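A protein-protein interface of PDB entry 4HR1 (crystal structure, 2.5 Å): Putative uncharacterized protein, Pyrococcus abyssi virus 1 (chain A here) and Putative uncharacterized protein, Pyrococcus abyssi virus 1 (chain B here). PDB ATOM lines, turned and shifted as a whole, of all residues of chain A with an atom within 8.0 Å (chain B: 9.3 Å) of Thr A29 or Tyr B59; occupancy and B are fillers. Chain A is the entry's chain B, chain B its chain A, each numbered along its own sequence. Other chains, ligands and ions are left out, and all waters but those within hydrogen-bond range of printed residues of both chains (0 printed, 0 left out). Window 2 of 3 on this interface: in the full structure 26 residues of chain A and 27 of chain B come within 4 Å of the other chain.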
ATOM      1  N   THR A  18     -28.249   0.345  24.018  1.00  0.00           N
ATOM      2  CA  THR A  18     -27.916  -0.831  23.209  1.00  0.00           C
ATOM      3  C   THR A  18     -28.733  -0.812  21.932  1.00  0.00           C
ATOM      4  O   THR A  18     -28.204  -1.157  20.879  1.00  0.00           O
ATOM      5  CB  THR A  18     -28.122  -2.136  24.035  1.00  0.00           C
ATOM      6  OG1 THR A  18     -27.288  -2.077  25.190  1.00  0.00           O
ATOM      7  CG2 THR A  18     -27.779  -3.399  23.254  1.00  0.00           C
ATOM      8  N   ALA A  19     -30.028  -0.420  22.019  1.00  0.00           N
ATOM      9  CA  ALA A  19     -30.913  -0.323  20.854  1.00  0.00           C
ATOM     10  C   ALA A  19     -30.393   0.769  19.886  1.00  0.00           C
ATOM     11  O   ALA A  19     -30.375   0.558  18.674  1.00  0.00           O
ATOM     12  CB  ALA A  19     -32.330  -0.029  21.296  1.00  0.00           C
ATOM     13  N   ALA A  21     -27.200   1.681  19.691  1.00  0.00           N
ATOM     14  CA  ALA A  21     -25.964   1.072  19.211  1.00  0.00           C
ATOM     15  C   ALA A  21     -26.299   0.107  18.090  1.00  0.00           C
ATOM     16  O   ALA A  21     -25.613   0.072  17.074  1.00  0.00           O
ATOM     17  CB  ALA A  21     -25.259   0.343  20.349  1.00  0.00           C
ATOM     18  N   PHE A  22     -27.397  -0.623  18.255  1.00  0.00           N
ATOM     19  CA  PHE A  22     -27.910  -1.547  17.265  1.00  0.00           C
ATOM     20  C   PHE A  22     -28.380  -0.762  16.008  1.00  0.00           C
ATOM     21  O   PHE A  22     -28.175  -1.248  14.897  1.00  0.00           O
ATOM     22  CB  PHE A  22     -29.040  -2.381  17.895  1.00  0.00           C
ATOM     23  CG  PHE A  22     -29.747  -3.365  16.994  1.00  0.00           C
ATOM     24  CD1 PHE A  22     -30.954  -3.034  16.383  1.00  0.00           C
ATOM     25  CD2 PHE A  22     -29.243  -4.648  16.804  1.00  0.00           C
ATOM     26  CE1 PHE A  22     -31.617  -3.948  15.549  1.00  0.00           C
ATOM     27  CE2 PHE A  22     -29.903  -5.558  15.965  1.00  0.00           C
ATOM     28  CZ  PHE A  22     -31.091  -5.202  15.347  1.00  0.00           C
ATOM     29  N   LEU A  23     -28.992   0.445  16.182  1.00  0.00           N
ATOM     30  CA  LEU A  23     -29.478   1.260  15.049  1.00  0.00           C
ATOM     31  C   LEU A  23     -28.319   1.873  14.286  1.00  0.00           C
ATOM     32  O   LEU A  23     -28.294   1.788  13.067  1.00  0.00           O
ATOM     33  CB  LEU A  23     -30.497   2.352  15.466  1.00  0.00           C
ATOM     34  CG  LEU A  23     -31.888   1.879  15.877  1.00  0.00           C
ATOM     35  CD1 LEU A  23     -32.588   2.940  16.678  1.00  0.00           C
ATOM     36  CD2 LEU A  23     -32.722   1.464  14.668  1.00  0.00           C
ATOM     37  N   LYS A  24     -27.351   2.445  15.000  1.00  0.00           N
ATOM     38  CA  LYS A  24     -26.134   3.004  14.419  1.00  0.00           C
ATOM     39  C   LYS A  24     -25.318   1.902  13.701  1.00  0.00           C
ATOM     40  O   LYS A  24     -24.701   2.163  12.660  1.00  0.00           O
ATOM     41  CB  LYS A  24     -25.275   3.677  15.506  1.00  0.00           C
ATOM     42  CG  LYS A  24     -25.856   4.977  16.020  1.00  0.00           C
ATOM     43  CD  LYS A  24     -24.806   5.818  16.694  1.00  0.00           C
ATOM     44  CE  LYS A  24     -25.409   7.069  17.261  1.00  0.00           C
ATOM     45  NZ  LYS A  24     -24.370   8.085  17.579  1.00  0.00           N
ATOM     46  N   GLY A  25     -25.355   0.692  14.266  1.00  0.00           N
ATOM     47  CA  GLY A  25     -24.682  -0.493  13.746  1.00  0.00           C
ATOM     48  C   GLY A  25     -25.217  -0.923  12.403  1.00  0.00           C
ATOM     49  O   GLY A  25     -24.437  -1.231  11.503  1.00  0.00           O
ATOM     50  N   TYR A  26     -26.552  -0.943  12.267  1.00  0.00           N
ATOM     51  CA  TYR A  26     -27.277  -1.285  11.041  1.00  0.00           C
ATOM     52  C   TYR A  26     -27.041  -0.240   9.942  1.00  0.00           C
ATOM     53  O   TYR A  26     -26.834  -0.602   8.786  1.00  0.00           O
ATOM     54  CB  TYR A  26     -28.771  -1.388  11.363  1.00  0.00           C
ATOM     55  CG  TYR A  26     -29.710  -1.335  10.178  1.00  0.00           C
ATOM     56  CD1 TYR A  26     -30.068  -2.496   9.495  1.00  0.00           C
ATOM     57  CD2 TYR A  26     -30.331  -0.144   9.806  1.00  0.00           C
ATOM     58  CE1 TYR A  26     -31.014  -2.472   8.470  1.00  0.00           C
ATOM     59  CE2 TYR A  26     -31.243  -0.100   8.751  1.00  0.00           C
ATOM     60  CZ  TYR A  26     -31.593  -1.272   8.097  1.00  0.00           C
ATOM     61  OH  TYR A  26     -32.505  -1.248   7.074  1.00  0.00           O
ATOM     62  N   MET A  27     -27.128   1.052  10.315  1.00  0.00           N
ATOM     63  CA  MET A  27     -26.960   2.195   9.422  1.00  0.00           C
ATOM     64  C   MET A  27     -25.595   2.227   8.766  1.00  0.00           C
ATOM     65  O   MET A  27     -25.504   2.624   7.611  1.00  0.00           O
ATOM     66  CB  MET A  27     -27.242   3.509  10.160  1.00  0.00           C
ATOM     67  CG  MET A  27     -28.711   3.810  10.265  1.00  0.00           C
ATOM     68  SD  MET A  27     -29.069   5.238  11.300  1.00  0.00           S
ATOM     69  CE  MET A  27     -30.800   5.242  11.142  1.00  0.00           C
ATOM     70  N   GLU A  28     -24.541   1.810   9.493  1.00  0.00           N
ATOM     71  CA  GLU A  28     -23.168   1.733   8.986  1.00  0.00           C
ATOM     72  C   GLU A  28     -23.080   0.747   7.802  1.00  0.00           C
ATOM     73  O   GLU A  28     -22.485   1.068   6.769  1.00  0.00           O
ATOM     74  CB  GLU A  28     -22.228   1.276  10.104  1.00  0.00           C
ATOM     75  CG  GLU A  28     -21.410   2.395  10.708  1.00  0.00           C
ATOM     76  CD  GLU A  28     -20.269   1.870  11.554  1.00  0.00           C
ATOM     77  OE1 GLU A  28     -19.133   1.792  11.030  1.00  0.00           O
ATOM     78  OE2 GLU A  28     -20.522   1.477  12.717  1.00  0.00           O
ATOM     79  N   THR A  29     -23.697  -0.441   7.962  1.00  0.00           N
ATOM     80  CA  THR A  29     -23.708  -1.503   6.961  1.00  0.00           C
ATOM     81  C   THR A  29     -24.519  -1.084   5.741  1.00  0.00           C
ATOM     82  O   THR A  29     -23.966  -1.020   4.640  1.00  0.00           O
ATOM     83  CB  THR A  29     -24.156  -2.875   7.559  1.00  0.00           C
ATOM     84  OG1 THR A  29     -25.581  -2.989   7.573  1.00  0.00           O
ATOM     85  CG2 THR A  29     -23.570  -3.160   8.945  1.00  0.00           C
ATOM     86  N   THR A  30     -25.809  -0.758   5.945  1.00  0.00           N
ATOM     87  CA  THR A  30     -26.746  -0.366   4.886  1.00  0.00           C
ATOM     88  C   THR A  30     -26.469   0.997   4.230  1.00  0.00           C
ATOM     89  O   THR A  30     -26.982   1.259   3.131  1.00  0.00           O
ATOM     90  CB  THR A  30     -28.202  -0.455   5.386  1.00  0.00           C
ATOM     91  OG1 THR A  30     -28.445   0.561   6.365  1.00  0.00           O
ATOM     92  CG2 THR A  30     -28.551  -1.837   5.929  1.00  0.00           C
ATOM     93  N   GLY A  31     -25.708   1.851   4.917  1.00  0.00           N
ATOM     94  CA  GLY A  31     -25.447   3.219   4.486  1.00  0.00           C
ATOM     95  C   GLY A  31     -26.587   4.124   4.924  1.00  0.00           C
ATOM     96  O   GLY A  31     -27.764   3.763   4.782  1.00  0.00           O
ATOM     97  N   ALA A  32     -26.259   5.292   5.493  1.00  0.00           N
ATOM     98  CA  ALA A  32     -27.293   6.222   5.939  1.00  0.00           C
ATOM     99  C   ALA A  32     -27.021   7.659   5.495  1.00  0.00           C
ATOM    100  O   ALA A  32     -25.871   8.005   5.208  1.00  0.00           O
ATOM    101  CB  ALA A  32     -27.444   6.158   7.457  1.00  0.00           C
ATOM    102  N   GLY A 100     -36.640   0.281   8.304  1.00  0.00           N
ATOM    103  CA  GLY A 100     -36.802  -1.009   7.640  1.00  0.00           C
ATOM    104  C   GLY A 100     -36.124  -2.208   8.268  1.00  0.00           C
ATOM    105  O   GLY A 100     -36.041  -3.260   7.623  1.00  0.00           O
ATOM    106  N   LEU A 101     -35.663  -2.077   9.535  1.00  0.00           N
ATOM    107  CA  LEU A 101     -35.020  -3.151  10.301  1.00  0.00           C
ATOM    108  C   LEU A 101     -36.002  -4.283  10.625  1.00  0.00           C
ATOM    109  O   LEU A 101     -35.599  -5.443  10.735  1.00  0.00           O
ATOM    110  CB  LEU A 101     -34.424  -2.599  11.596  1.00  0.00           C
ATOM    111  CG  LEU A 101     -32.930  -2.649  11.693  1.00  0.00           C
ATOM    112  CD1 LEU A 101     -32.453  -1.794  12.817  1.00  0.00           C
ATOM    113  CD2 LEU A 101     -32.432  -4.090  11.828  1.00  0.00           C
ATOM    114  N   ILE A 111     -35.981  -8.420  17.781  1.00  0.00           N
ATOM    115  CA  ILE A 111     -34.915  -7.454  17.996  1.00  0.00           C
ATOM    116  C   ILE A 111     -34.811  -7.124  19.494  1.00  0.00           C
ATOM    117  O   ILE A 111     -33.698  -7.085  20.025  1.00  0.00           O
ATOM    118  CB  ILE A 111     -35.094  -6.209  17.087  1.00  0.00           C
ATOM    119  CG1 ILE A 111     -34.833  -6.571  15.609  1.00  0.00           C
ATOM    120  CG2 ILE A 111     -34.190  -5.060  17.544  1.00  0.00           C
ATOM    121  CD1 ILE A 111     -35.303  -5.521  14.575  1.00  0.00           C
ATOM    122  N   TYR A 114     -33.297  -9.975  21.451  1.00  0.00           N
ATOM    123  CA  TYR A 114     -31.857  -9.935  21.197  1.00  0.00           C
ATOM    124  C   TYR A 114     -31.215  -8.846  22.065  1.00  0.00           C
ATOM    125  O   TYR A 114     -30.103  -9.020  22.534  1.00  0.00           O
ATOM    126  CB  TYR A 114     -31.563  -9.691  19.694  1.00  0.00           C
ATOM    127  CG  TYR A 114     -30.096  -9.416  19.413  1.00  0.00           C
ATOM    128  CD1 TYR A 114     -29.154 -10.448  19.440  1.00  0.00           C
ATOM    129  CD2 TYR A 114     -29.639  -8.119  19.180  1.00  0.00           C
ATOM    130  CE1 TYR A 114     -27.797 -10.194  19.250  1.00  0.00           C
ATOM    131  CE2 TYR A 114     -28.280  -7.851  19.004  1.00  0.00           C
ATOM    132  CZ  TYR A 114     -27.365  -8.895  19.027  1.00  0.00           C
ATOM    133  OH  TYR A 114     -26.026  -8.658  18.859  1.00  0.00           O
ATOM    134  N   LEU A 115     -31.905  -7.726  22.264  1.00  0.00           N
ATOM    135  CA  LEU A 115     -31.362  -6.625  23.057  1.00  0.00           C
ATOM    136  C   LEU A 115     -31.417  -6.943  24.546  1.00  0.00           C
ATOM    137  O   LEU A 115     -30.487  -6.592  25.283  1.00  0.00           O
ATOM    138  CB  LEU A 115     -32.060  -5.287  22.716  1.00  0.00           C
ATOM    139  CG  LEU A 115     -31.953  -4.816  21.243  1.00  0.00           C
ATOM    140  CD1 LEU A 115     -33.014  -3.794  20.916  1.00  0.00           C
ATOM    141  CD2 LEU A 115     -30.547  -4.300  20.896  1.00  0.00           C
ATOM    142  N   LEU A 118     -28.577  -9.267  25.493  1.00  0.00           N
ATOM    143  CA  LEU A 118     -27.289  -8.579  25.573  1.00  0.00           C
ATOM    144  C   LEU A 118     -27.116  -7.873  26.900  1.00  0.00           C
ATOM    145  O   LEU A 118     -25.989  -7.692  27.368  1.00  0.00           O
ATOM    146  CB  LEU A 118     -27.192  -7.556  24.428  1.00  0.00           C
ATOM    147  CG  LEU A 118     -26.361  -7.938  23.203  1.00  0.00           C
ATOM    148  CD1 LEU A 118     -26.687  -9.333  22.678  1.00  0.00           C
ATOM    149  CD2 LEU A 118     -26.569  -6.939  22.103  1.00  0.00           C
ATOM    150  N   ALA B   6     -21.034  -9.528  21.543  1.00  0.00           N
ATOM    151  CA  ALA B   6     -21.973  -8.426  21.818  1.00  0.00           C
ATOM    152  C   ALA B   6     -22.307  -8.301  23.299  1.00  0.00           C
ATOM    153  O   ALA B   6     -22.076  -7.235  23.878  1.00  0.00           O
ATOM    154  CB  ALA B   6     -23.240  -8.558  20.972  1.00  0.00           C
ATOM    155  N   VAL B   9     -19.085  -6.974  25.392  1.00  0.00           N
ATOM    156  CA  VAL B   9     -18.835  -5.526  25.268  1.00  0.00           C
ATOM    157  C   VAL B   9     -19.927  -4.678  25.941  1.00  0.00           C
ATOM    158  O   VAL B   9     -19.606  -3.723  26.643  1.00  0.00           O
ATOM    159  CB  VAL B   9     -18.461  -5.063  23.827  1.00  0.00           C
ATOM    160  CG1 VAL B   9     -17.339  -5.927  23.248  1.00  0.00           C
ATOM    161  CG2 VAL B   9     -19.667  -5.069  22.898  1.00  0.00           C
ATOM    162  N   ILE B  10     -21.200  -5.080  25.787  1.00  0.00           N
ATOM    163  CA  ILE B  10     -22.351  -4.416  26.396  1.00  0.00           C
ATOM    164  C   ILE B  10     -22.236  -4.420  27.923  1.00  0.00           C
ATOM    165  O   ILE B  10     -22.333  -3.351  28.531  1.00  0.00           O
ATOM    166  CB  ILE B  10     -23.720  -4.960  25.838  1.00  0.00           C
ATOM    167  CG1 ILE B  10     -23.950  -4.537  24.343  1.00  0.00           C
ATOM    168  CG2 ILE B  10     -24.913  -4.519  26.715  1.00  0.00           C
ATOM    169  CD1 ILE B  10     -23.594  -2.925  24.014  1.00  0.00           C
ATOM    170  N   VAL B  54     -17.467  -0.221  18.790  1.00  0.00           N
ATOM    171  CA  VAL B  54     -18.017  -1.583  18.820  1.00  0.00           C
ATOM    172  C   VAL B  54     -19.496  -1.774  18.420  1.00  0.00           C
ATOM    173  O   VAL B  54     -19.937  -2.924  18.295  1.00  0.00           O
ATOM    174  CB  VAL B  54     -17.646  -2.336  20.127  1.00  0.00           C
ATOM    175  CG1 VAL B  54     -16.138  -2.525  20.246  1.00  0.00           C
ATOM    176  CG2 VAL B  54     -18.211  -1.637  21.364  1.00  0.00           C
ATOM    177  N   ASN B  55     -20.246  -0.663  18.191  1.00  0.00           N
ATOM    178  CA  ASN B  55     -21.664  -0.636  17.770  1.00  0.00           C
ATOM    179  C   ASN B  55     -21.930  -1.563  16.611  1.00  0.00           C
ATOM    180  O   ASN B  55     -23.027  -2.125  16.496  1.00  0.00           O
ATOM    181  CB  ASN B  55     -22.081   0.776  17.316  1.00  0.00           C
ATOM    182  CG  ASN B  55     -22.179   1.827  18.387  1.00  0.00           C
ATOM    183  OD1 ASN B  55     -22.252   1.535  19.591  1.00  0.00           O
ATOM    184  ND2 ASN B  55     -22.219   3.090  17.951  1.00  0.00           N
ATOM    185  N   TRP B  56     -20.936  -1.683  15.707  1.00  0.00           N
ATOM    186  CA  TRP B  56     -21.035  -2.550  14.543  1.00  0.00           C
ATOM    187  C   TRP B  56     -21.357  -3.970  14.974  1.00  0.00           C
ATOM    188  O   TRP B  56     -22.238  -4.579  14.374  1.00  0.00           O
ATOM    189  CB  TRP B  56     -19.752  -2.475  13.700  1.00  0.00           C
ATOM    190  CG  TRP B  56     -18.516  -2.956  14.397  1.00  0.00           C
ATOM    191  CD1 TRP B  56     -17.647  -2.208  15.143  1.00  0.00           C
ATOM    192  CD2 TRP B  56     -18.016  -4.299  14.422  1.00  0.00           C
ATOM    193  NE1 TRP B  56     -16.645  -3.006  15.644  1.00  0.00           N
ATOM    194  CE2 TRP B  56     -16.866  -4.303  15.242  1.00  0.00           C
ATOM    195  CE3 TRP B  56     -18.453  -5.511  13.858  1.00  0.00           C
ATOM    196  CZ2 TRP B  56     -16.126  -5.466  15.483  1.00  0.00           C
ATOM    197  CZ3 TRP B  56     -17.738  -6.671  14.129  1.00  0.00           C
ATOM    198  CH2 TRP B  56     -16.588  -6.640  14.923  1.00  0.00           C
ATOM    199  N   ASP B  57     -20.714  -4.462  16.087  1.00  0.00           N
ATOM    200  CA  ASP B  57     -20.912  -5.821  16.578  1.00  0.00           C
ATOM    201  C   ASP B  57     -22.263  -6.088  17.221  1.00  0.00           C
ATOM    202  O   ASP B  57     -22.783  -7.214  17.121  1.00  0.00           O
ATOM    203  CB  ASP B  57     -19.735  -6.327  17.413  1.00  0.00           C
ATOM    204  CG  ASP B  57     -19.728  -7.837  17.533  1.00  0.00           C
ATOM    205  OD1 ASP B  57     -19.650  -8.338  18.678  1.00  0.00           O
ATOM    206  OD2 ASP B  57     -19.944  -8.522  16.496  1.00  0.00           O
ATOM    207  N   VAL B  58     -22.867  -5.044  17.814  1.00  0.00           N
ATOM    208  CA  VAL B  58     -24.206  -5.124  18.377  1.00  0.00           C
ATOM    209  C   VAL B  58     -25.180  -5.488  17.238  1.00  0.00           C
ATOM    210  O   VAL B  58     -25.904  -6.467  17.386  1.00  0.00           O
ATOM    211  CB  VAL B  58     -24.585  -3.841  19.142  1.00  0.00           C
ATOM    212  CG1 VAL B  58     -25.931  -3.992  19.852  1.00  0.00           C
ATOM    213  CG2 VAL B  58     -23.486  -3.456  20.129  1.00  0.00           C
ATOM    214  N   TYR B  59     -25.105  -4.794  16.058  1.00  0.00           N
ATOM    215  CA  TYR B  59     -25.923  -5.175  14.898  1.00  0.00           C
ATOM    216  C   TYR B  59     -25.386  -6.416  14.199  1.00  0.00           C
ATOM    217  O   TYR B  59     -26.175  -7.333  13.921  1.00  0.00           O
ATOM    218  CB  TYR B  59     -26.137  -4.049  13.838  1.00  0.00           C
ATOM    219  CG  TYR B  59     -26.948  -4.553  12.647  1.00  0.00           C
ATOM    220  CD1 TYR B  59     -28.244  -5.037  12.818  1.00  0.00           C
ATOM    221  CD2 TYR B  59     -26.370  -4.678  11.385  1.00  0.00           C
ATOM    222  CE1 TYR B  59     -28.956  -5.599  11.757  1.00  0.00           C
ATOM    223  CE2 TYR B  59     -27.088  -5.202  10.304  1.00  0.00           C
ATOM    224  CZ  TYR B  59     -28.382  -5.668  10.498  1.00  0.00           C
ATOM    225  OH  TYR B  59     -29.093  -6.228   9.461  1.00  0.00           O
ATOM    226  N   ALA B  60     -24.065  -6.420  13.859  1.00  0.00           N
ATOM    227  CA  ALA B  60     -23.426  -7.518  13.128  1.00  0.00           C
ATOM    228  C   ALA B  60     -23.782  -8.895  13.668  1.00  0.00           C
ATOM    229  O   ALA B  60     -24.247  -9.738  12.894  1.00  0.00           O
ATOM    230  CB  ALA B  60     -21.915  -7.326  13.055  1.00  0.00           C
ATOM    231  N   GLN B  61     -23.684  -9.077  15.005  1.00  0.00           N
ATOM    232  CA  GLN B  61     -24.010 -10.348  15.651  1.00  0.00           C
ATOM    233  C   GLN B  61     -25.449 -10.797  15.373  1.00  0.00           C
ATOM    234  O   GLN B  61     -25.658 -11.956  14.997  1.00  0.00           O
ATOM    235  CB  GLN B  61     -23.685 -10.324  17.160  1.00  0.00           C
ATOM    236  CG  GLN B  61     -23.562 -11.716  17.785  1.00  0.00           C
ATOM    237  CD  GLN B  61     -23.100 -11.681  19.224  1.00  0.00           C
ATOM    238  OE1 GLN B  61     -23.861 -11.981  20.155  1.00  0.00           O
ATOM    239  NE2 GLN B  61     -21.830 -11.345  19.435  1.00  0.00           N
ATOM    240  N   TYR B  62     -26.427  -9.872  15.520  1.00  0.00           N
ATOM    241  CA  TYR B  62     -27.848 -10.140  15.274  1.00  0.00           C
ATOM    242  C   TYR B  62     -28.067 -10.580  13.834  1.00  0.00           C
ATOM    243  O   TYR B  62     -28.751 -11.580  13.604  1.00  0.00           O
ATOM    244  CB  TYR B  62     -28.713  -8.899  15.606  1.00  0.00           C
ATOM    245  CG  TYR B  62     -30.158  -9.018  15.155  1.00  0.00           C
ATOM    246  CD1 TYR B  62     -31.073  -9.796  15.867  1.00  0.00           C
ATOM    247  CD2 TYR B  62     -30.597  -8.407  13.980  1.00  0.00           C
ATOM    248  CE1 TYR B  62     -32.390  -9.952  15.427  1.00  0.00           C
ATOM    249  CE2 TYR B  62     -31.913  -8.551  13.534  1.00  0.00           C
ATOM    250  CZ  TYR B  62     -32.808  -9.325  14.260  1.00  0.00           C
ATOM    251  OH  TYR B  62     -34.110  -9.467  13.820  1.00  0.00           O
ATOM    252  N   ALA B  63     -27.492  -9.807  12.880  1.00  0.00           N
ATOM    253  CA  ALA B  63     -27.588  -9.972  11.426  1.00  0.00           C
ATOM    254  C   ALA B  63     -27.176 -11.346  10.908  1.00  0.00           C
ATOM    255  O   ALA B  63     -27.862 -11.878  10.032  1.00  0.00           O
ATOM    256  CB  ALA B  63     -26.795  -8.880  10.719  1.00  0.00           C
ATOM    257  N   ARG B  64     -26.066 -11.921  11.428  1.00  0.00           N
ATOM    258  CA  ARG B  64     -25.625 -13.243  10.976  1.00  0.00           C
ATOM    259  C   ARG B  64     -26.165 -14.428  11.778  1.00  0.00           C
ATOM    260  O   ARG B  64     -25.404 -15.272  12.255  1.00  0.00           O
ATOM    261  CB  ARG B  64     -24.130 -13.338  10.603  1.00  0.00           C
ATOM    262  CG  ARG B  64     -23.161 -12.531  11.448  1.00  0.00           C
ATOM    263  CD  ARG B  64     -22.506 -11.442  10.612  1.00  0.00           C
ATOM    264  NE  ARG B  64     -21.154 -11.126  11.081  1.00  0.00           N
ATOM    265  CZ  ARG B  64     -20.356 -10.218  10.526  1.00  0.00           C
ATOM    266  NH1 ARG B  64     -20.763  -9.518   9.475  1.00  0.00           N
ATOM    267  NH2 ARG B  64     -19.152  -9.996  11.023  1.00  0.00           N
ATOM    268  N   GLY B  65     -27.497 -14.465  11.889  1.00  0.00           N
ATOM    269  CA  GLY B  65     -28.273 -15.507  12.561  1.00  0.00           C
ATOM    270  C   GLY B  65     -27.958 -15.743  14.026  1.00  0.00           C
ATOM    271  O   GLY B  65     -28.053 -16.882  14.503  1.00  0.00           O
ATOM    272  N   ASP B  66     -27.580 -14.657  14.748  1.00  0.00           N
ATOM    273  CA  ASP B  66     -27.206 -14.650  16.172  1.00  0.00           C
ATOM    274  C   ASP B  66     -25.964 -15.540  16.504  1.00  0.00           C
ATOM    275  O   ASP B  66     -25.600 -15.697  17.678  1.00  0.00           O
ATOM    276  CB  ASP B  66     -28.432 -14.905  17.088  1.00  0.00           C
ATOM    277  CG  ASP B  66     -28.304 -14.455  18.537  1.00  0.00           C
ATOM    278  OD1 ASP B  66     -29.044 -14.990  19.390  1.00  0.00           O
ATOM    279  OD2 ASP B  66     -27.463 -13.568  18.817  1.00  0.00           O
ATOM    280  N   PHE B  67     -25.292 -16.073  15.454  1.00  0.00           N
ATOM    281  CA  PHE B  67     -24.085 -16.887  15.581  1.00  0.00           C
ATOM    282  C   PHE B  67     -22.901 -15.977  15.854  1.00  0.00           C
ATOM    283  O   PHE B  67     -22.844 -14.874  15.303  1.00  0.00           O
ATOM    284  CB  PHE B  67     -23.801 -17.670  14.284  1.00  0.00           C
ATOM    285  CG  PHE B  67     -24.832 -18.677  13.827  1.00  0.00           C
ATOM    286  CD1 PHE B  67     -25.283 -19.676  14.686  1.00  0.00           C
ATOM    287  CD2 PHE B  67     -25.285 -18.680  12.513  1.00  0.00           C
ATOM    288  CE1 PHE B  67     -26.218 -20.622  14.254  1.00  0.00           C
ATOM    289  CE2 PHE B  67     -26.213 -19.632  12.079  1.00  0.00           C
ATOM    290  CZ  PHE B  67     -26.672 -20.597  12.952  1.00  0.00           C
ATOM    291  N   GLU B  74     -12.093  -8.636  12.767  1.00  0.00           N
ATOM    292  CA  GLU B  74     -13.209  -8.204  13.614  1.00  0.00           C
ATOM    293  C   GLU B  74     -12.921  -8.580  15.073  1.00  0.00           C
ATOM    294  O   GLU B  74     -12.835  -7.686  15.925  1.00  0.00           O
ATOM    295  CB  GLU B  74     -14.514  -8.849  13.137  1.00  0.00           C
ATOM    296  CG  GLU B  74     -15.163  -8.178  11.937  1.00  0.00           C
ATOM    297  CD  GLU B  74     -16.263  -8.990  11.279  1.00  0.00           C
ATOM    298  OE1 GLU B  74     -16.542 -10.120  11.744  1.00  0.00           O
ATOM    299  OE2 GLU B  74     -16.834  -8.505  10.275  1.00  0.00           O
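Of the printed residues of chain B, Ala A21 touches Asn B55. Of chain B, only Val B58 (3.8 Å), Tyr B59 (3.6 Å) and Tyr B62 (3.5 Å) come within 4 Å of Phe A22. Gly A25 touches just these residues of chain B: Asn B55 and Tyr B59. Printed residues of chain B within 4 Å of Thr A29: Tyr B59 (3.8 Å). No residue of chain B comes within 4 Å of Thr A30. Gly A100 touches none of the printed residues of chain B. Of the printed residues of chain B, Tyr A114 touches Ala B6 (3.5 Å), Asp B57 (3.95 Å), Val B58 (2.6 Å), Gln B61 (3.3 Å), Tyr B62 (3.6 Å) and Asp B66 (3.4 Å). Of the printed residues of chain A, Ala B6 touches Tyr A114 (3.5 Å) and Leu A118 (3.9 Å). Trp B56 touches none of the printed residues of chain A. Of chain A, only Phe A22 (3.6 Å), Gly A25 (3.6 Å), Tyr A26 (3.5 Å), Thr A29 (3.8 Å) and Leu A101 (3.8 Å) come within 4 Å of Tyr B59. Of the printed residues of chain A, Gln B61 touches Tyr A114. Printed residues of chain A within 4 Å of Asp B66: Tyr A114 (3.4 Å). The nearest residue of chain A that does not touch Tyr B59 is Tyr A114 (4.9 Å).
Val B58 touches Thr A18 (CG1 to O, 3.8 Å). O of Val B58 touches CD2 of Phe A22, at 3.8 Å. Phe A22 touches Tyr B59 (CE2 to CD1, 3.6 Å). CA of Gly A25 touches O of Asn B55, 3.6 Å away. Tyr B59 touches Leu A101 (CE1 to CD2, 3.8 Å). CB of Gln B61 touches OH of Tyr A114, at 3.3 Å. N of Tyr B62 touches OH of Tyr A114 (3.6 Å). Tyr A114 touches Asp B66 (CE1 to OD2, 3.4 Å). Leu A118 touches Ile B10 (O to CG2, 3.4 Å). CD2 of Leu A118 touches CG1 of Val B58 (3.8 Å).
The backbone carbonyl oxygen of Ala A21 lies close to the backbone carbonyl oxygen of Asn B55 (3.4 Å). O of Val B58 sits at hydrogen-bond distance from OH of Tyr A114, 2.6 Å away.
The backbone NH (N) of Ala B6 lies close to the side-chain amide nitrogen (NE2) of Gln B61 (2.9 Å). The side-chain hydroxyl (OG1) of Thr A29 lies within hydrogen-bond range of the backbone carbonyl oxygen (O) of Tyr A26 (3.0 Å). The side-chain carboxylate (OD1) of Asp B57 sits at hydrogen-bond distance from the backbone NH (N) of Ala B6 (3.4 Å). OG1 of Thr A30 is in hydrogen-bond range of O of Tyr A26, 3.1 Å away. The backbone NH (N) of Asp B66 sits close to the backbone carbonyl oxygen (O) of Gln B61.
Hydrophobic or aromatic side chains of chain A that line the printed part of chain B: Ala A21, Phe A22, Tyr A26, Leu A101, Ile A111, Tyr A114 and Leu A118. Of the 18 printed residues of chain B, 9 touch a printed residue of chain A.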
